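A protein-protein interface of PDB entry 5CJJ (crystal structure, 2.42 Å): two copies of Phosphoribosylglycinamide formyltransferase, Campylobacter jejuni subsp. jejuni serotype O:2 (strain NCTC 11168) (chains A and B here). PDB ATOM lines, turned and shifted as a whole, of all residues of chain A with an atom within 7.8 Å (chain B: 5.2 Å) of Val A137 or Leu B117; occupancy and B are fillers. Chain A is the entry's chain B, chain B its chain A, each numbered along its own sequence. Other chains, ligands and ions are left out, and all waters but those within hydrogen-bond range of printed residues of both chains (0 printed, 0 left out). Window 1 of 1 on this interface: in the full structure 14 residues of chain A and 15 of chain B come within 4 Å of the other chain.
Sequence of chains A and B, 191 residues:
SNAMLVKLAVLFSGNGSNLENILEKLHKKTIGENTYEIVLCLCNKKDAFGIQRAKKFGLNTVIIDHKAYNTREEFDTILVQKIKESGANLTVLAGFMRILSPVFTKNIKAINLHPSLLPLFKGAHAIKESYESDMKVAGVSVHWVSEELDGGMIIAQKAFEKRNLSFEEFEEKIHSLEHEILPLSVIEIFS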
ATOM      1  N   LEU A 117      12.171 -18.076   5.296  1.00  0.00           N
ATOM      2  CA  LEU A 117      13.002 -18.151   4.103  1.00  0.00           C
ATOM      3  C   LEU A 117      14.471 -18.241   4.502  1.00  0.00           C
ATOM      4  O   LEU A 117      15.157 -17.225   4.602  1.00  0.00           O
ATOM      5  CB  LEU A 117      12.771 -16.935   3.207  1.00  0.00           C
ATOM      6  CG  LEU A 117      11.357 -16.735   2.661  1.00  0.00           C
ATOM      7  CD1 LEU A 117      11.256 -15.408   1.926  1.00  0.00           C
ATOM      8  CD2 LEU A 117      10.961 -17.882   1.747  1.00  0.00           C
ATOM      9  N   LEU A 120      17.427 -17.039   6.614  1.00  0.00           N
ATOM     10  CA  LEU A 120      16.875 -16.017   7.497  1.00  0.00           C
ATOM     11  C   LEU A 120      16.021 -16.613   8.612  1.00  0.00           C
ATOM     12  O   LEU A 120      15.352 -17.628   8.420  1.00  0.00           O
ATOM     13  CB  LEU A 120      16.051 -14.997   6.710  1.00  0.00           C
ATOM     14  CG  LEU A 120      16.811 -14.112   5.726  1.00  0.00           C
ATOM     15  CD1 LEU A 120      15.849 -13.162   5.037  1.00  0.00           C
ATOM     16  CD2 LEU A 120      17.912 -13.346   6.436  1.00  0.00           C
ATOM     17  N   PHE A 121      16.064 -15.972   9.774  1.00  0.00           N
ATOM     18  CA  PHE A 121      15.208 -16.317  10.908  1.00  0.00           C
ATOM     19  C   PHE A 121      15.328 -17.767  11.379  1.00  0.00           C
ATOM     20  O   PHE A 121      14.324 -18.454  11.556  1.00  0.00           O
ATOM     21  CB  PHE A 121      13.742 -15.979  10.609  1.00  0.00           C
ATOM     22  CG  PHE A 121      13.522 -14.556  10.193  1.00  0.00           C
ATOM     23  CD1 PHE A 121      13.716 -13.525  11.093  1.00  0.00           C
ATOM     24  CD2 PHE A 121      13.115 -14.249   8.906  1.00  0.00           C
ATOM     25  CE1 PHE A 121      13.517 -12.217  10.718  1.00  0.00           C
ATOM     26  CE2 PHE A 121      12.913 -12.940   8.525  1.00  0.00           C
ATOM     27  CZ  PHE A 121      13.114 -11.923   9.433  1.00  0.00           C
ATOM     28  N   SER A 130       9.631 -12.901  11.474  1.00  0.00           N
ATOM     29  CA  SER A 130       9.427 -12.648  10.051  1.00  0.00           C
ATOM     30  C   SER A 130       8.221 -11.746   9.816  1.00  0.00           C
ATOM     31  O   SER A 130       8.128 -11.075   8.787  1.00  0.00           O
ATOM     32  CB  SER A 130       9.264 -13.960   9.280  1.00  0.00           C
ATOM     33  OG  SER A 130       8.215 -14.742   9.822  1.00  0.00           O
ATOM     34  N   TYR A 131       7.297 -11.733  10.770  1.00  0.00           N
ATOM     35  CA  TYR A 131       6.123 -10.877  10.675  1.00  0.00           C
ATOM     36  C   TYR A 131       6.448  -9.451  11.103  1.00  0.00           C
ATOM     37  O   TYR A 131       6.060  -8.491  10.439  1.00  0.00           O
ATOM     38  CB  TYR A 131       4.975 -11.429  11.521  1.00  0.00           C
ATOM     39  CG  TYR A 131       3.748 -10.545  11.520  1.00  0.00           C
ATOM     40  CD1 TYR A 131       2.921 -10.477  10.408  1.00  0.00           C
ATOM     41  CD2 TYR A 131       3.417  -9.779  12.630  1.00  0.00           C
ATOM     42  CE1 TYR A 131       1.799  -9.672  10.398  1.00  0.00           C
ATOM     43  CE2 TYR A 131       2.295  -8.969  12.631  1.00  0.00           C
ATOM     44  CZ  TYR A 131       1.490  -8.920  11.511  1.00  0.00           C
ATOM     45  OH  TYR A 131       0.372  -8.117  11.502  1.00  0.00           O
ATOM     46  N   SER A 133       9.319  -8.130  11.112  1.00  0.00           N
ATOM     47  CA  SER A 133      10.390  -7.610  10.269  1.00  0.00           C
ATOM     48  C   SER A 133       9.870  -6.598   9.255  1.00  0.00           C
ATOM     49  O   SER A 133       8.690  -6.600   8.907  1.00  0.00           O
ATOM     50  CB  SER A 133      11.106  -8.750   9.542  1.00  0.00           C
ATOM     51  OG  SER A 133      12.038  -8.241   8.602  1.00  0.00           O
ATOM     52  N   ASP A 134      10.760  -5.731   8.781  1.00  0.00           N
ATOM     53  CA  ASP A 134      10.391  -4.729   7.790  1.00  0.00           C
ATOM     54  C   ASP A 134      10.379  -5.328   6.385  1.00  0.00           C
ATOM     55  O   ASP A 134      10.148  -4.625   5.402  1.00  0.00           O
ATOM     56  CB  ASP A 134      11.337  -3.528   7.852  1.00  0.00           C
ATOM     57  CG  ASP A 134      12.771  -3.895   7.531  1.00  0.00           C
ATOM     58  OD1 ASP A 134      13.185  -5.030   7.847  1.00  0.00           O
ATOM     59  OD2 ASP A 134      13.489  -3.046   6.963  1.00  0.00           O
ATOM     60  N   MET A 135      10.637  -6.631   6.302  1.00  0.00           N
ATOM     61  CA  MET A 135      10.568  -7.347   5.036  1.00  0.00           C
ATOM     62  C   MET A 135       9.128  -7.411   4.554  1.00  0.00           C
ATOM     63  O   MET A 135       8.201  -7.515   5.357  1.00  0.00           O
ATOM     64  CB  MET A 135      11.134  -8.762   5.178  1.00  0.00           C
ATOM     65  CG  MET A 135      12.632  -8.819   5.412  1.00  0.00           C
ATOM     66  SD  MET A 135      13.332 -10.633   5.305  1.00  0.00           S
ATOM     67  CE  MET A 135      12.976 -10.970   3.416  1.00  0.00           C
ATOM     68  N   LYS A 136       8.944  -7.352   3.239  1.00  0.00           N
ATOM     69  CA  LYS A 136       7.606  -7.368   2.661  1.00  0.00           C
ATOM     70  C   LYS A 136       7.244  -8.741   2.107  1.00  0.00           C
ATOM     71  O   LYS A 136       6.152  -8.938   1.579  1.00  0.00           O
ATOM     72  CB  LYS A 136       7.470  -6.288   1.586  1.00  0.00           C
ATOM     73  CG  LYS A 136       7.736  -4.891   2.117  1.00  0.00           C
ATOM     74  CD  LYS A 136       6.933  -4.636   3.384  1.00  0.00           C
ATOM     75  CE  LYS A 136       7.353  -3.344   4.065  1.00  0.00           C
ATOM     76  NZ  LYS A 136       6.694  -3.188   5.392  1.00  0.00           N
ATOM     77  N   VAL A 137       8.167  -9.689   2.236  1.00  0.00           N
ATOM     78  CA  VAL A 137       7.897 -11.073   1.863  1.00  0.00           C
ATOM     79  C   VAL A 137       8.344 -12.030   2.963  1.00  0.00           C
ATOM     80  O   VAL A 137       9.223 -11.711   3.761  1.00  0.00           O
ATOM     81  CB  VAL A 137       8.578 -11.465   0.534  1.00  0.00           C
ATOM     82  CG1 VAL A 137       8.039 -10.629  -0.616  1.00  0.00           C
ATOM     83  CG2 VAL A 137      10.091 -11.327   0.642  1.00  0.00           C
ATOM     84  N   ALA A 138       7.722 -13.202   2.998  1.00  0.00           N
ATOM     85  CA  ALA A 138       8.096 -14.256   3.932  1.00  0.00           C
ATOM     86  C   ALA A 138       7.778 -15.595   3.287  1.00  0.00           C
ATOM     87  O   ALA A 138       7.353 -15.643   2.135  1.00  0.00           O
ATOM     88  CB  ALA A 138       7.347 -14.101   5.242  1.00  0.00           C
ATOM     89  N   GLY A 139       7.979 -16.683   4.022  1.00  0.00           N
ATOM     90  CA  GLY A 139       7.686 -18.000   3.489  1.00  0.00           C
ATOM     91  C   GLY A 139       8.166 -19.153   4.346  1.00  0.00           C
ATOM     92  O   GLY A 139       8.281 -19.033   5.566  1.00  0.00           O
ATOM     93  N   GLN A 157      11.715 -24.163  -1.254  1.00  0.00           N
ATOM     94  CA  GLN A 157      11.321 -22.886  -0.667  1.00  0.00           C
ATOM     95  C   GLN A 157      10.116 -22.295  -1.398  1.00  0.00           C
ATOM     96  O   GLN A 157      10.010 -22.396  -2.621  1.00  0.00           O
ATOM     97  CB  GLN A 157      12.486 -21.888  -0.697  1.00  0.00           C
ATOM     98  CG  GLN A 157      13.497 -22.046   0.432  1.00  0.00           C
ATOM     99  CD  GLN A 157      14.575 -20.976   0.413  1.00  0.00           C
ATOM    100  OE1 GLN A 157      14.941 -20.462  -0.645  1.00  0.00           O
ATOM    101  NE2 GLN A 157      15.084 -20.631   1.590  1.00  0.00           N
ATOM    102  N   ALA A 159       7.514 -18.595  -1.205  1.00  0.00           N
ATOM    103  CA  ALA A 159       7.340 -17.280  -0.603  1.00  0.00           C
ATOM    104  C   ALA A 159       5.974 -16.674  -0.899  1.00  0.00           C
ATOM    105  O   ALA A 159       5.371 -16.946  -1.935  1.00  0.00           O
ATOM    106  CB  ALA A 159       8.448 -16.334  -1.057  1.00  0.00           C
ATOM    107  N   PHE A 160       5.496 -15.847   0.022  1.00  0.00           N
ATOM    108  CA  PHE A 160       4.268 -15.096  -0.187  1.00  0.00           C
ATOM    109  C   PHE A 160       4.504 -13.646   0.203  1.00  0.00           C
ATOM    110  O   PHE A 160       5.343 -13.354   1.052  1.00  0.00           O
ATOM    111  CB  PHE A 160       3.119 -15.681   0.639  1.00  0.00           C
ATOM    112  CG  PHE A 160       3.308 -15.548   2.123  1.00  0.00           C
ATOM    113  CD1 PHE A 160       4.087 -16.457   2.816  1.00  0.00           C
ATOM    114  CD2 PHE A 160       2.698 -14.522   2.827  1.00  0.00           C
ATOM    115  CE1 PHE A 160       4.263 -16.341   4.179  1.00  0.00           C
ATOM    116  CE2 PHE A 160       2.870 -14.402   4.191  1.00  0.00           C
ATOM    117  CZ  PHE A 160       3.654 -15.314   4.867  1.00  0.00           C
ATOM    118  N   GLU A 161       3.764 -12.740  -0.421  1.00  0.00           N
ATOM    119  CA  GLU A 161       3.886 -11.327  -0.099  1.00  0.00           C
ATOM    120  C   GLU A 161       3.097 -10.994   1.161  1.00  0.00           C
ATOM    121  O   GLU A 161       1.944 -11.398   1.309  1.00  0.00           O
ATOM    122  CB  GLU A 161       3.437 -10.467  -1.278  1.00  0.00           C
ATOM    123  CG  GLU A 161       4.339 -10.608  -2.492  1.00  0.00           C
ATOM    124  CD  GLU A 161       3.986  -9.639  -3.600  1.00  0.00           C
ATOM    125  OE1 GLU A 161       4.715  -8.638  -3.772  1.00  0.00           O
ATOM    126  OE2 GLU A 161       2.982  -9.878  -4.303  1.00  0.00           O
ATOM    127  N   LYS A 162       3.734 -10.263   2.069  1.00  0.00           N
ATOM    128  CA  LYS A 162       3.143  -9.970   3.367  1.00  0.00           C
ATOM    129  C   LYS A 162       1.897  -9.094   3.236  1.00  0.00           C
ATOM    130  O   LYS A 162       0.874  -9.369   3.865  1.00  0.00           O
ATOM    131  CB  LYS A 162       4.176  -9.322   4.294  1.00  0.00           C
ATOM    132  CG  LYS A 162       4.089  -9.802   5.735  1.00  0.00           C
ATOM    133  CD  LYS A 162       5.436  -9.726   6.443  1.00  0.00           C
ATOM    134  CE  LYS A 162       5.651  -8.379   7.113  1.00  0.00           C
ATOM    135  NZ  LYS A 162       6.906  -8.362   7.917  1.00  0.00           N
ATOM    136  N   ARG A 163       1.993  -8.052   2.414  1.00  0.00           N
ATOM    137  CA  ARG A 163       0.875  -7.143   2.147  1.00  0.00           C
ATOM    138  C   ARG A 163       0.212  -6.585   3.412  1.00  0.00           C
ATOM    139  O   ARG A 163       0.796  -5.750   4.103  1.00  0.00           O
ATOM    140  CB  ARG A 163      -0.152  -7.798   1.213  1.00  0.00           C
ATOM    141  CG  ARG A 163       0.393  -8.067  -0.187  1.00  0.00           C
ATOM    142  CD  ARG A 163      -0.707  -8.383  -1.190  1.00  0.00           C
ATOM    143  NE  ARG A 163      -0.266  -8.161  -2.566  1.00  0.00           N
ATOM    144  CZ  ARG A 163       0.147  -9.119  -3.391  1.00  0.00           C
ATOM    145  NH1 ARG A 163       0.173 -10.382  -2.986  1.00  0.00           N
ATOM    146  NH2 ARG A 163       0.531  -8.813  -4.622  1.00  0.00           N
ATOM    147  N   PHE A 170      -1.244 -14.162   9.072  1.00  0.00           N
ATOM    148  CA  PHE A 170       0.117 -14.427   8.626  1.00  0.00           C
ATOM    149  C   PHE A 170       0.500 -15.859   8.971  1.00  0.00           C
ATOM    150  O   PHE A 170       1.053 -16.585   8.145  1.00  0.00           O
ATOM    151  CB  PHE A 170       1.081 -13.450   9.299  1.00  0.00           C
ATOM    152  CG  PHE A 170       2.506 -13.578   8.837  1.00  0.00           C
ATOM    153  CD1 PHE A 170       2.950 -12.894   7.718  1.00  0.00           C
ATOM    154  CD2 PHE A 170       3.407 -14.361   9.538  1.00  0.00           C
ATOM    155  CE1 PHE A 170       4.259 -13.000   7.301  1.00  0.00           C
ATOM    156  CE2 PHE A 170       4.716 -14.472   9.125  1.00  0.00           C
ATOM    157  CZ  PHE A 170       5.143 -13.791   8.006  1.00  0.00           C
ATOM    158  N   PRO B 115      18.819  -5.802  -6.317  1.00  0.00           N
ATOM    159  CA  PRO B 115      18.385  -7.021  -7.008  1.00  0.00           C
ATOM    160  C   PRO B 115      18.439  -8.273  -6.136  1.00  0.00           C
ATOM    161  O   PRO B 115      18.845  -9.331  -6.617  1.00  0.00           O
ATOM    162  CB  PRO B 115      19.393  -7.138  -8.148  1.00  0.00           C
ATOM    163  CG  PRO B 115      20.631  -6.536  -7.598  1.00  0.00           C
ATOM    164  CD  PRO B 115      20.179  -5.399  -6.719  1.00  0.00           C
ATOM    165  N   SER B 116      18.032  -8.159  -4.876  1.00  0.00           N
ATOM    166  CA  SER B 116      17.973  -9.314  -3.991  1.00  0.00           C
ATOM    167  C   SER B 116      16.926  -9.105  -2.906  1.00  0.00           C
ATOM    168  O   SER B 116      16.473  -7.986  -2.677  1.00  0.00           O
ATOM    169  CB  SER B 116      19.339  -9.577  -3.352  1.00  0.00           C
ATOM    170  OG  SER B 116      19.420  -8.991  -2.065  1.00  0.00           O
ATOM    171  N   LEU B 117      16.544 -10.190  -2.244  1.00  0.00           N
ATOM    172  CA  LEU B 117      15.613 -10.109  -1.129  1.00  0.00           C
ATOM    173  C   LEU B 117      16.355  -9.699   0.136  1.00  0.00           C
ATOM    174  O   LEU B 117      16.784 -10.551   0.911  1.00  0.00           O
ATOM    175  CB  LEU B 117      14.910 -11.448  -0.913  1.00  0.00           C
ATOM    176  CG  LEU B 117      13.963 -11.920  -2.017  1.00  0.00           C
ATOM    177  CD1 LEU B 117      13.450 -13.320  -1.718  1.00  0.00           C
ATOM    178  CD2 LEU B 117      12.803 -10.950  -2.182  1.00  0.00           C
ATOM    179  N   LEU B 118      16.508  -8.393   0.330  1.00  0.00           N
ATOM    180  CA  LEU B 118      17.184  -7.856   1.507  1.00  0.00           C
ATOM    181  C   LEU B 118      16.547  -8.374   2.797  1.00  0.00           C
ATOM    182  O   LEU B 118      15.337  -8.599   2.842  1.00  0.00           O
ATOM    183  CB  LEU B 118      17.163  -6.327   1.468  1.00  0.00           C
ATOM    184  CG  LEU B 118      18.059  -5.684   0.409  1.00  0.00           C
ATOM    185  CD1 LEU B 118      17.798  -4.193   0.329  1.00  0.00           C
ATOM    186  CD2 LEU B 118      19.518  -5.953   0.728  1.00  0.00           C
ATOM    187  N   PRO B 119      17.358  -8.557   3.855  1.00  0.00           N
ATOM    188  CA  PRO B 119      18.785  -8.222   3.956  1.00  0.00           C
ATOM    189  C   PRO B 119      19.732  -9.254   3.338  1.00  0.00           C
ATOM    190  O   PRO B 119      20.946  -9.130   3.509  1.00  0.00           O
ATOM    191  CB  PRO B 119      19.008  -8.164   5.466  1.00  0.00           C
ATOM    192  CG  PRO B 119      18.053  -9.168   6.002  1.00  0.00           C
ATOM    193  CD  PRO B 119      16.830  -9.077   5.130  1.00  0.00           C
ATOM    194  N   LEU B 120      19.195 -10.249   2.639  1.00  0.00           N
ATOM    195  CA  LEU B 120      20.032 -11.258   1.999  1.00  0.00           C
ATOM    196  C   LEU B 120      20.795 -10.678   0.816  1.00  0.00           C
ATOM    197  O   LEU B 120      20.276  -9.836   0.083  1.00  0.00           O
ATOM    198  CB  LEU B 120      19.197 -12.449   1.526  1.00  0.00           C
ATOM    199  CG  LEU B 120      18.567 -13.338   2.593  1.00  0.00           C
ATOM    200  CD1 LEU B 120      17.473 -14.190   1.976  1.00  0.00           C
ATOM    201  CD2 LEU B 120      19.623 -14.211   3.253  1.00  0.00           C
ATOM    202  N   VAL B 137      14.264 -19.451  -3.893  1.00  0.00           N
ATOM    203  CA  VAL B 137      13.571 -18.216  -4.239  1.00  0.00           C
ATOM    204  C   VAL B 137      14.542 -17.041  -4.293  1.00  0.00           C
ATOM    205  O   VAL B 137      15.585 -17.049  -3.641  1.00  0.00           O
ATOM    206  CB  VAL B 137      12.439 -17.892  -3.246  1.00  0.00           C
ATOM    207  CG1 VAL B 137      11.405 -19.005  -3.235  1.00  0.00           C
ATOM    208  CG2 VAL B 137      13.004 -17.664  -1.851  1.00  0.00           C
ATOM    209  N   ALA B 138      14.187 -16.037  -5.086  1.00  0.00           N
ATOM    210  CA  ALA B 138      14.978 -14.822  -5.202  1.00  0.00           C
ATOM    211  C   ALA B 138      14.034 -13.654  -5.437  1.00  0.00           C
ATOM    212  O   ALA B 138      12.816 -13.829  -5.441  1.00  0.00           O
ATOM    213  CB  ALA B 138      15.973 -14.943  -6.340  1.00  0.00           C
ATOM    214  N   GLY B 139      14.588 -12.464  -5.635  1.00  0.00           N
ATOM    215  CA  GLY B 139      13.762 -11.300  -5.894  1.00  0.00           C
ATOM    216  C   GLY B 139      14.507  -9.982  -5.930  1.00  0.00           C
ATOM    217  O   GLY B 139      15.719  -9.945  -6.136  1.00  0.00           O
ATOM    218  N   VAL B 140      13.768  -8.893  -5.742  1.00  0.00           N
ATOM    219  CA  VAL B 140      14.339  -7.553  -5.746  1.00  0.00           C
ATOM    220  C   VAL B 140      13.783  -6.758  -4.577  1.00  0.00           C
ATOM    221  O   VAL B 140      12.710  -7.067  -4.069  1.00  0.00           O
ATOM    222  CB  VAL B 140      14.007  -6.806  -7.052  1.00  0.00           C
ATOM    223  CG1 VAL B 140      14.736  -7.437  -8.227  1.00  0.00           C
ATOM    224  CG2 VAL B 140      12.504  -6.796  -7.286  1.00  0.00           C
ATOM    225  N   SER B 141      14.512  -5.733  -4.153  1.00  0.00           N
ATOM    226  CA  SER B 141      14.074  -4.928  -3.019  1.00  0.00           C
ATOM    227  C   SER B 141      14.243  -3.431  -3.253  1.00  0.00           C
ATOM    228  O   SER B 141      15.151  -2.996  -3.961  1.00  0.00           O
ATOM    229  CB  SER B 141      14.822  -5.343  -1.748  1.00  0.00           C
ATOM    230  OG  SER B 141      14.509  -6.675  -1.376  1.00  0.00           O
ATOM    231  N   GLN B 157       9.370  -5.338  -1.644  1.00  0.00           N
ATOM    232  CA  GLN B 157      10.125  -6.406  -2.287  1.00  0.00           C
ATOM    233  C   GLN B 157       9.220  -7.490  -2.864  1.00  0.00           C
ATOM    234  O   GLN B 157       8.198  -7.843  -2.277  1.00  0.00           O
ATOM    235  CB  GLN B 157      11.167  -7.000  -1.336  1.00  0.00           C
ATOM    236  CG  GLN B 157      10.694  -7.205   0.086  1.00  0.00           C
ATOM    237  CD  GLN B 157      11.818  -7.651   0.999  1.00  0.00           C
ATOM    238  OE1 GLN B 157      11.582  -8.113   2.112  1.00  0.00           O
ATOM    239  NE2 GLN B 157      13.053  -7.516   0.528  1.00  0.00           N
ATOM    240  N   LYS B 158       9.604  -8.000  -4.030  1.00  0.00           N
ATOM    241  CA  LYS B 158       8.842  -9.040  -4.709  1.00  0.00           C
ATOM    242  C   LYS B 158       9.688 -10.298  -4.854  1.00  0.00           C
ATOM    243  O   LYS B 158      10.864 -10.223  -5.201  1.00  0.00           O
ATOM    244  CB  LYS B 158       8.385  -8.553  -6.085  1.00  0.00           C
ATOM    245  N   ALA B 159       9.088 -11.452  -4.587  1.00  0.00           N
ATOM    246  CA  ALA B 159       9.816 -12.713  -4.646  1.00  0.00           C
ATOM    247  C   ALA B 159       9.274 -13.636  -5.730  1.00  0.00           C
ATOM    248  O   ALA B 159       8.081 -13.624  -6.034  1.00  0.00           O
ATOM    249  CB  ALA B 159       9.784 -13.410  -3.293  1.00  0.00           C
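OE1 of Gln A157 sits at hydrogen-bond distance from N of Val B137 (3.5 Å). The side-chain amide oxygen of Gln B157 is in hydrogen-bond range of the backbone NH of Lys A136 (3.0 Å). O of Leu B118 sits close to SD of Met A135 (3.8 Å).
The side-chain hydroxyl of Ser B116 is in hydrogen-bond range of the backbone carbonyl oxygen of Leu B120. The side-chain hydroxyl (OG) of Ser B141 sits at hydrogen-bond distance from the side-chain amide nitrogen (NE2) of Gln B157. The backbone carbonyl oxygen (O) of Lys A136 sits at hydrogen-bond distance from the backbone NH (N) of Lys A162, at 2.8 Å. NH2 of Arg A163 lies within salt-bridge range of OE2 of Glu A161 (2.7 Å). The side-chain hydroxyl (OG) of Ser B141 is in hydrogen-bond range of the backbone NH (N) of Leu B118, 3.1 Å away. O of Met A135 sits at hydrogen-bond distance from NZ of Lys A162 (3.0 Å).
Leu A120 touches Leu B120. Met A135 touches Pro B119. Gln B157 touches Met A135. CG2 of Val A137 touches CD2 of Leu B117, at 3.9 Å. O of Gln B157 touches CG1 of Val A137, 3.2 Å away. CB of Ala B159 touches CB of Ala A159, 3.9 Å away. Glu A161 touches Gln B157 (OE1 to O, 3.9 Å).
Val A137 touches two residues of chain B. Leu B117 touches just one residue of chain A: Val A137 (3.9 Å). Of the printed residues of chain B, Met A135 touches Leu B118 (3.4 Å), Pro B119 (3.8 Å) and Gln B157 (3.2 Å). Of the printed residues of chain B, Lys A136 touches Gln B157 (3.0 Å). Of the printed residues of chain A, Ala B159 touches Ala A159 (3.9 Å). Of the printed residues of chain A, Leu B120 touches Leu A120 (3.6 Å). The nearest residue of chain B that does not touch Val A137 is Ala B159 (4.2 Å).
Of the 14 printed residues of chain B, 7 touch a printed residue of chain A. Hydrophobic or aromatic side chains of chain B within 4 Å of the printed part of chain A: Leu B117, Pro B119, Leu B120, Val B137 and Ala B159. Among the printed residues, 10 pairs touch across the chains.
Leu A120 touches its own counterpart, Leu B120. Val A137 touches Leu B117, but with the chains exchanged Leu A117 does not touch Val B137 (4.1 Å). Val A137 touches Gln B157, and with the chains exchanged Gln A157 touches Val B137. Ala B159 touches its own counterpart, Ala A159. 7 positions are printed for both chains. Of the 10 pairs that touch across the chains among the printed residues, 4 have their exchanged pair printed and touching as well.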
